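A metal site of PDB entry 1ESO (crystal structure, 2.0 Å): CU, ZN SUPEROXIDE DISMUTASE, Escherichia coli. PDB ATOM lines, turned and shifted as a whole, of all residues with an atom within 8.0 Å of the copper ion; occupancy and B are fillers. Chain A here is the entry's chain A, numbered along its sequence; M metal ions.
The copper ion is bound by NE2 of His 50, NE2 of His 128 and ND1 of His 48.
Slightly farther from the copper ion lies NE2 of His 73 (2.7 Å).
The nearest printed residue that does not touch the copper ion is Met 126 (4.3 Å).
N of His 50 lies within hydrogen-bond range of O of Ala 124 (2.7 Å).
The backbone NH of His 128 sits at hydrogen-bond distance from the backbone carbonyl oxygen of Gly 46.
The backbone carbonyl oxygen of His 48 is in hydrogen-bond range of the backbone NH of Met 126 (2.8 Å).
ND1 of His 50 is in hydrogen-bond range of O of Gly 71.
A ring nitrogen (NE2) of His 73 sits close to a ring nitrogen (ND1) of His 48.
A ring nitrogen (ND1) of His 50 sits close to the backbone carbonyl oxygen (O) of Gly 72.
OD2 of Asp 132 lies within hydrogen-bond range of NE2 of His 48 (2.8 Å).
O of Gly 145 sits at hydrogen-bond distance from ND1 of His 128 (3.1 Å).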
ATOM      1  N   GLY A  46      16.295  17.285 -19.980  1.00  0.00           N
ATOM      2  CA  GLY A  46      15.403  16.199 -19.593  1.00  0.00           C
ATOM      3  C   GLY A  46      14.359  16.783 -18.662  1.00  0.00           C
ATOM      4  O   GLY A  46      14.694  17.512 -17.715  1.00  0.00           O
ATOM      5  N   PHE A  47      13.127  16.437 -18.959  1.00  0.00           N
ATOM      6  CA  PHE A  47      11.949  16.941 -18.241  1.00  0.00           C
ATOM      7  C   PHE A  47      11.031  15.750 -17.948  1.00  0.00           C
ATOM      8  O   PHE A  47      10.354  15.223 -18.839  1.00  0.00           O
ATOM      9  CB  PHE A  47      11.266  17.933 -19.186  1.00  0.00           C
ATOM     10  CG  PHE A  47      10.278  18.896 -18.535  1.00  0.00           C
ATOM     11  CD1 PHE A  47      10.497  19.395 -17.243  1.00  0.00           C
ATOM     12  CD2 PHE A  47       9.149  19.288 -19.254  1.00  0.00           C
ATOM     13  CE1 PHE A  47       9.587  20.287 -16.669  1.00  0.00           C
ATOM     14  CE2 PHE A  47       8.231  20.193 -18.687  1.00  0.00           C
ATOM     15  CZ  PHE A  47       8.446  20.683 -17.394  1.00  0.00           C
ATOM     16  N   HIS A  48      11.000  15.330 -16.686  1.00  0.00           N
ATOM     17  CA  HIS A  48      10.179  14.173 -16.278  1.00  0.00           C
ATOM     18  C   HIS A  48       9.551  14.347 -14.900  1.00  0.00           C
ATOM     19  O   HIS A  48      10.027  15.137 -14.076  1.00  0.00           O
ATOM     20  CB  HIS A  48      11.033  12.903 -16.164  1.00  0.00           C
ATOM     21  CG  HIS A  48      12.177  12.802 -17.182  1.00  0.00           C
ATOM     22  ND1 HIS A  48      13.518  12.784 -16.792  1.00  0.00           N
ATOM     23  CD2 HIS A  48      12.183  12.703 -18.538  1.00  0.00           C
ATOM     24  CE1 HIS A  48      14.262  12.682 -17.875  1.00  0.00           C
ATOM     25  NE2 HIS A  48      13.478  12.633 -18.925  1.00  0.00           N
ATOM     26  N   ILE A  49       8.491  13.587 -14.715  1.00  0.00           N
ATOM     27  CA  ILE A  49       7.773  13.488 -13.432  1.00  0.00           C
ATOM     28  C   ILE A  49       8.326  12.248 -12.735  1.00  0.00           C
ATOM     29  O   ILE A  49       8.350  11.150 -13.307  1.00  0.00           O
ATOM     30  CB  ILE A  49       6.258  13.341 -13.664  1.00  0.00           C
ATOM     31  CG1 ILE A  49       5.641  14.502 -14.460  1.00  0.00           C
ATOM     32  CG2 ILE A  49       5.464  13.264 -12.361  1.00  0.00           C
ATOM     33  CD1 ILE A  49       4.118  14.388 -14.579  1.00  0.00           C
ATOM     34  N   HIS A  50       8.778  12.417 -11.511  1.00  0.00           N
ATOM     35  CA  HIS A  50       9.368  11.298 -10.744  1.00  0.00           C
ATOM     36  C   HIS A  50       8.291  10.724  -9.791  1.00  0.00           C
ATOM     37  O   HIS A  50       7.257  11.360  -9.532  1.00  0.00           O
ATOM     38  CB  HIS A  50      10.646  11.764 -10.059  1.00  0.00           C
ATOM     39  CG  HIS A  50      11.816  11.860 -11.060  1.00  0.00           C
ATOM     40  ND1 HIS A  50      12.997  11.130 -10.910  1.00  0.00           N
ATOM     41  CD2 HIS A  50      11.972  12.573 -12.219  1.00  0.00           C
ATOM     42  CE1 HIS A  50      13.800  11.410 -11.923  1.00  0.00           C
ATOM     43  NE2 HIS A  50      13.205  12.270 -12.707  1.00  0.00           N
ATOM     44  N   GLY A  71      13.060   9.453  -6.218  1.00  0.00           N
ATOM     45  CA  GLY A  71      13.027   8.115  -6.841  1.00  0.00           C
ATOM     46  C   GLY A  71      13.181   8.223  -8.375  1.00  0.00           C
ATOM     47  O   GLY A  71      13.651   9.246  -8.899  1.00  0.00           O
ATOM     48  N   GLY A  72      12.778   7.153  -9.054  1.00  0.00           N
ATOM     49  CA  GLY A  72      12.874   7.051 -10.529  1.00  0.00           C
ATOM     50  C   GLY A  72      11.699   7.758 -11.218  1.00  0.00           C
ATOM     51  O   GLY A  72      10.941   8.525 -10.592  1.00  0.00           O
ATOM     52  N   HIS A  73      11.561   7.508 -12.500  1.00  0.00           N
ATOM     53  CA  HIS A  73      10.497   8.104 -13.313  1.00  0.00           C
ATOM     54  C   HIS A  73       9.162   7.415 -12.989  1.00  0.00           C
ATOM     55  O   HIS A  73       9.088   6.196 -12.861  1.00  0.00           O
ATOM     56  CB  HIS A  73      10.801   7.926 -14.796  1.00  0.00           C
ATOM     57  CG  HIS A  73      11.957   8.785 -15.286  1.00  0.00           C
ATOM     58  ND1 HIS A  73      12.400   8.746 -16.607  1.00  0.00           N
ATOM     59  CD2 HIS A  73      12.749   9.689 -14.645  1.00  0.00           C
ATOM     60  CE1 HIS A  73      13.412   9.597 -16.724  1.00  0.00           C
ATOM     61  NE2 HIS A  73      13.621  10.166 -15.562  1.00  0.00           N
ATOM     62  N   LEU A  74       8.122   8.239 -12.864  1.00  0.00           N
ATOM     63  CA  LEU A  74       6.756   7.765 -12.598  1.00  0.00           C
ATOM     64  C   LEU A  74       6.381   6.700 -13.619  1.00  0.00           C
ATOM     65  O   LEU A  74       6.473   6.902 -14.835  1.00  0.00           O
ATOM     66  CB  LEU A  74       5.789   8.938 -12.741  1.00  0.00           C
ATOM     67  CG  LEU A  74       4.333   8.516 -12.695  1.00  0.00           C
ATOM     68  CD1 LEU A  74       3.894   8.116 -11.281  1.00  0.00           C
ATOM     69  CD2 LEU A  74       3.383   9.615 -13.148  1.00  0.00           C
ATOM     70  N   HIS A  82      12.260   3.550 -20.706  1.00  0.00           N
ATOM     71  CA  HIS A  82      12.265   4.996 -20.942  1.00  0.00           C
ATOM     72  C   HIS A  82      12.117   5.254 -22.438  1.00  0.00           C
ATOM     73  O   HIS A  82      13.063   5.070 -23.218  1.00  0.00           O
ATOM     74  CB  HIS A  82      13.563   5.631 -20.486  1.00  0.00           C
ATOM     75  CG  HIS A  82      13.500   7.142 -20.670  1.00  0.00           C
ATOM     76  ND1 HIS A  82      12.726   7.943 -19.833  1.00  0.00           N
ATOM     77  CD2 HIS A  82      14.077   7.970 -21.580  1.00  0.00           C
ATOM     78  CE1 HIS A  82      12.856   9.194 -20.236  1.00  0.00           C
ATOM     79  NE2 HIS A  82      13.653   9.225 -21.276  1.00  0.00           N
ATOM     80  N   HIS A  90       7.641   4.759 -19.316  1.00  0.00           N
ATOM     81  CA  HIS A  90       7.312   5.565 -18.130  1.00  0.00           C
ATOM     82  C   HIS A  90       6.255   6.607 -18.495  1.00  0.00           C
ATOM     83  O   HIS A  90       6.401   7.360 -19.465  1.00  0.00           O
ATOM     84  CB  HIS A  90       8.519   6.363 -17.618  1.00  0.00           C
ATOM     85  CG  HIS A  90       9.794   5.557 -17.380  1.00  0.00           C
ATOM     86  ND1 HIS A  90      11.037   6.026 -17.804  1.00  0.00           N
ATOM     87  CD2 HIS A  90      10.038   4.362 -16.779  1.00  0.00           C
ATOM     88  CE1 HIS A  90      11.953   5.139 -17.471  1.00  0.00           C
ATOM     89  NE2 HIS A  90      11.369   4.139 -16.850  1.00  0.00           N
ATOM     90  N   GLY A  92       5.663   9.098 -16.882  1.00  0.00           N
ATOM     91  CA  GLY A  92       6.205  10.386 -16.420  1.00  0.00           C
ATOM     92  C   GLY A  92       7.099  11.095 -17.455  1.00  0.00           C
ATOM     93  O   GLY A  92       7.524  12.248 -17.248  1.00  0.00           O
ATOM     94  N   ASP A  93       7.375  10.436 -18.557  1.00  0.00           N
ATOM     95  CA  ASP A  93       8.238  11.003 -19.624  1.00  0.00           C
ATOM     96  C   ASP A  93       7.527  12.154 -20.355  1.00  0.00           C
ATOM     97  O   ASP A  93       6.490  11.960 -21.002  1.00  0.00           O
ATOM     98  CB  ASP A  93       8.559   9.938 -20.688  1.00  0.00           C
ATOM     99  CG  ASP A  93       9.331   8.725 -20.145  1.00  0.00           C
ATOM    100  OD1 ASP A  93       9.707   8.688 -18.908  1.00  0.00           O
ATOM    101  OD2 ASP A  93       9.600   7.737 -20.928  1.00  0.00           O
ATOM    102  N   ALA A 124       6.991  14.626  -8.088  1.00  0.00           N
ATOM    103  CA  ALA A 124       8.042  15.637  -8.315  1.00  0.00           C
ATOM    104  C   ALA A 124       8.292  15.881  -9.821  1.00  0.00           C
ATOM    105  O   ALA A 124       8.517  14.934 -10.584  1.00  0.00           O
ATOM    106  CB  ALA A 124       9.359  15.192  -7.681  1.00  0.00           C
ATOM    107  N   LEU A 125       8.245  17.165 -10.178  1.00  0.00           N
ATOM    108  CA  LEU A 125       8.575  17.669 -11.544  1.00  0.00           C
ATOM    109  C   LEU A 125      10.064  17.940 -11.539  1.00  0.00           C
ATOM    110  O   LEU A 125      10.543  18.719 -10.696  1.00  0.00           O
ATOM    111  CB  LEU A 125       7.848  18.994 -11.807  1.00  0.00           C
ATOM    112  CG  LEU A 125       7.266  19.191 -13.212  1.00  0.00           C
ATOM    113  CD1 LEU A 125       7.044  20.679 -13.564  1.00  0.00           C
ATOM    114  CD2 LEU A 125       8.083  18.608 -14.359  1.00  0.00           C
ATOM    115  N   MET A 126      10.760  17.327 -12.462  1.00  0.00           N
ATOM    116  CA  MET A 126      12.221  17.401 -12.483  1.00  0.00           C
ATOM    117  C   MET A 126      12.808  17.887 -13.828  1.00  0.00           C
ATOM    118  O   MET A 126      12.305  17.577 -14.905  1.00  0.00           O
ATOM    119  CB  MET A 126      12.779  16.004 -12.238  1.00  0.00           C
ATOM    120  CG  MET A 126      14.205  15.993 -11.729  1.00  0.00           C
ATOM    121  SD  MET A 126      14.304  16.135  -9.960  1.00  0.00           S
ATOM    122  CE  MET A 126      13.361  14.828  -9.196  1.00  0.00           C
ATOM    123  N   VAL A 127      13.899  18.638 -13.694  1.00  0.00           N
ATOM    124  CA  VAL A 127      14.697  19.127 -14.838  1.00  0.00           C
ATOM    125  C   VAL A 127      16.128  18.609 -14.679  1.00  0.00           C
ATOM    126  O   VAL A 127      16.748  18.771 -13.613  1.00  0.00           O
ATOM    127  CB  VAL A 127      14.726  20.655 -14.873  1.00  0.00           C
ATOM    128  CG1 VAL A 127      15.486  21.199 -16.086  1.00  0.00           C
ATOM    129  CG2 VAL A 127      13.337  21.273 -14.923  1.00  0.00           C
ATOM    130  N   HIS A 128      16.622  17.982 -15.742  1.00  0.00           N
ATOM    131  CA  HIS A 128      17.955  17.340 -15.748  1.00  0.00           C
ATOM    132  C   HIS A 128      19.007  18.208 -16.392  1.00  0.00           C
ATOM    133  O   HIS A 128      18.708  19.083 -17.210  1.00  0.00           O
ATOM    134  CB  HIS A 128      17.852  16.029 -16.514  1.00  0.00           C
ATOM    135  CG  HIS A 128      17.115  15.012 -15.676  1.00  0.00           C
ATOM    136  ND1 HIS A 128      17.794  14.143 -14.849  1.00  0.00           N
ATOM    137  CD2 HIS A 128      15.790  14.762 -15.527  1.00  0.00           C
ATOM    138  CE1 HIS A 128      16.902  13.413 -14.222  1.00  0.00           C
ATOM    139  NE2 HIS A 128      15.701  13.773 -14.617  1.00  0.00           N
ATOM    140  N   ASP A 132      17.499  14.584 -23.491  1.00  0.00           N
ATOM    141  CA  ASP A 132      16.652  13.382 -23.503  1.00  0.00           C
ATOM    142  C   ASP A 132      16.409  12.936 -24.943  1.00  0.00           C
ATOM    143  O   ASP A 132      15.712  13.611 -25.715  1.00  0.00           O
ATOM    144  CB  ASP A 132      15.309  13.659 -22.826  1.00  0.00           C
ATOM    145  CG  ASP A 132      14.542  12.375 -22.490  1.00  0.00           C
ATOM    146  OD1 ASP A 132      14.942  11.248 -22.968  1.00  0.00           O
ATOM    147  OD2 ASP A 132      13.500  12.424 -21.738  1.00  0.00           O
ATOM    148  N   LEU A 141      17.872   6.305 -19.205  1.00  0.00           N
ATOM    149  CA  LEU A 141      16.910   7.387 -18.972  1.00  0.00           C
ATOM    150  C   LEU A 141      17.089   8.572 -19.933  1.00  0.00           C
ATOM    151  O   LEU A 141      16.804   9.719 -19.570  1.00  0.00           O
ATOM    152  CB  LEU A 141      17.086   7.946 -17.563  1.00  0.00           C
ATOM    153  CG  LEU A 141      16.592   7.022 -16.456  1.00  0.00           C
ATOM    154  CD1 LEU A 141      15.981   5.725 -16.991  1.00  0.00           C
ATOM    155  CD2 LEU A 141      17.710   6.599 -15.501  1.00  0.00           C
ATOM    156  N   GLY A 144      19.843  11.842 -19.432  1.00  0.00           N
ATOM    157  CA  GLY A 144      19.429  12.961 -18.576  1.00  0.00           C
ATOM    158  C   GLY A 144      20.563  13.389 -17.627  1.00  0.00           C
ATOM    159  O   GLY A 144      20.849  14.578 -17.430  1.00  0.00           O
ATOM    160  N   GLY A 145      21.200  12.412 -17.016  1.00  0.00           N
ATOM    161  CA  GLY A 145      22.290  12.684 -16.063  1.00  0.00           C
ATOM    162  C   GLY A 145      21.713  13.255 -14.770  1.00  0.00           C
ATOM    163  O   GLY A 145      20.578  12.965 -14.394  1.00  0.00           O
ATOM    164  N   GLU A 146      22.502  14.086 -14.112  1.00  0.00           N
ATOM    165  CA  GLU A 146      22.132  14.659 -12.800  1.00  0.00           C
ATOM    166  C   GLU A 146      20.897  15.591 -12.873  1.00  0.00           C
ATOM    167  O   GLU A 146      20.602  16.197 -13.904  1.00  0.00           O
ATOM    168  CB  GLU A 146      23.316  15.397 -12.188  1.00  0.00           C
ATOM    169  N   ARG A 147      20.233  15.622 -11.716  1.00  0.00           N
ATOM    170  CA  ARG A 147      19.016  16.422 -11.453  1.00  0.00           C
ATOM    171  C   ARG A 147      19.431  17.860 -11.125  1.00  0.00           C
ATOM    172  O   ARG A 147      20.223  18.102 -10.212  1.00  0.00           O
ATOM    173  CB  ARG A 147      18.255  15.766 -10.292  1.00  0.00           C
ATOM    174  CG  ARG A 147      17.590  14.476 -10.741  1.00  0.00           C
ATOM    175  CD  ARG A 147      17.136  13.548  -9.617  1.00  0.00           C
ATOM    176  NE  ARG A 147      17.056  12.154 -10.088  1.00  0.00           N
ATOM    177  CZ  ARG A 147      16.353  11.167  -9.518  1.00  0.00           C
ATOM    178  NH1 ARG A 147      15.617  11.375  -8.418  1.00  0.00           N
ATOM    179  NH2 ARG A 147      16.323   9.924 -10.006  1.00  0.00           N
ATOM    180  N   ALA A 149      16.906  20.871 -11.355  1.00  0.00           N
ATOM    181  CA  ALA A 149      15.815  21.657 -10.734  1.00  0.00           C
ATOM    182  C   ALA A 149      14.612  20.759 -10.432  1.00  0.00           C
ATOM    183  O   ALA A 149      14.372  19.723 -11.062  1.00  0.00           O
ATOM    184  CB  ALA A 149      15.372  22.801 -11.660  1.00  0.00           C
HETATM  185 CU    CU M   1      13.919  12.635 -14.643  1.00  0.00          CU
HETATM  186 ZN    ZN M   2      11.483   7.833 -18.303  1.00  0.00          ZN
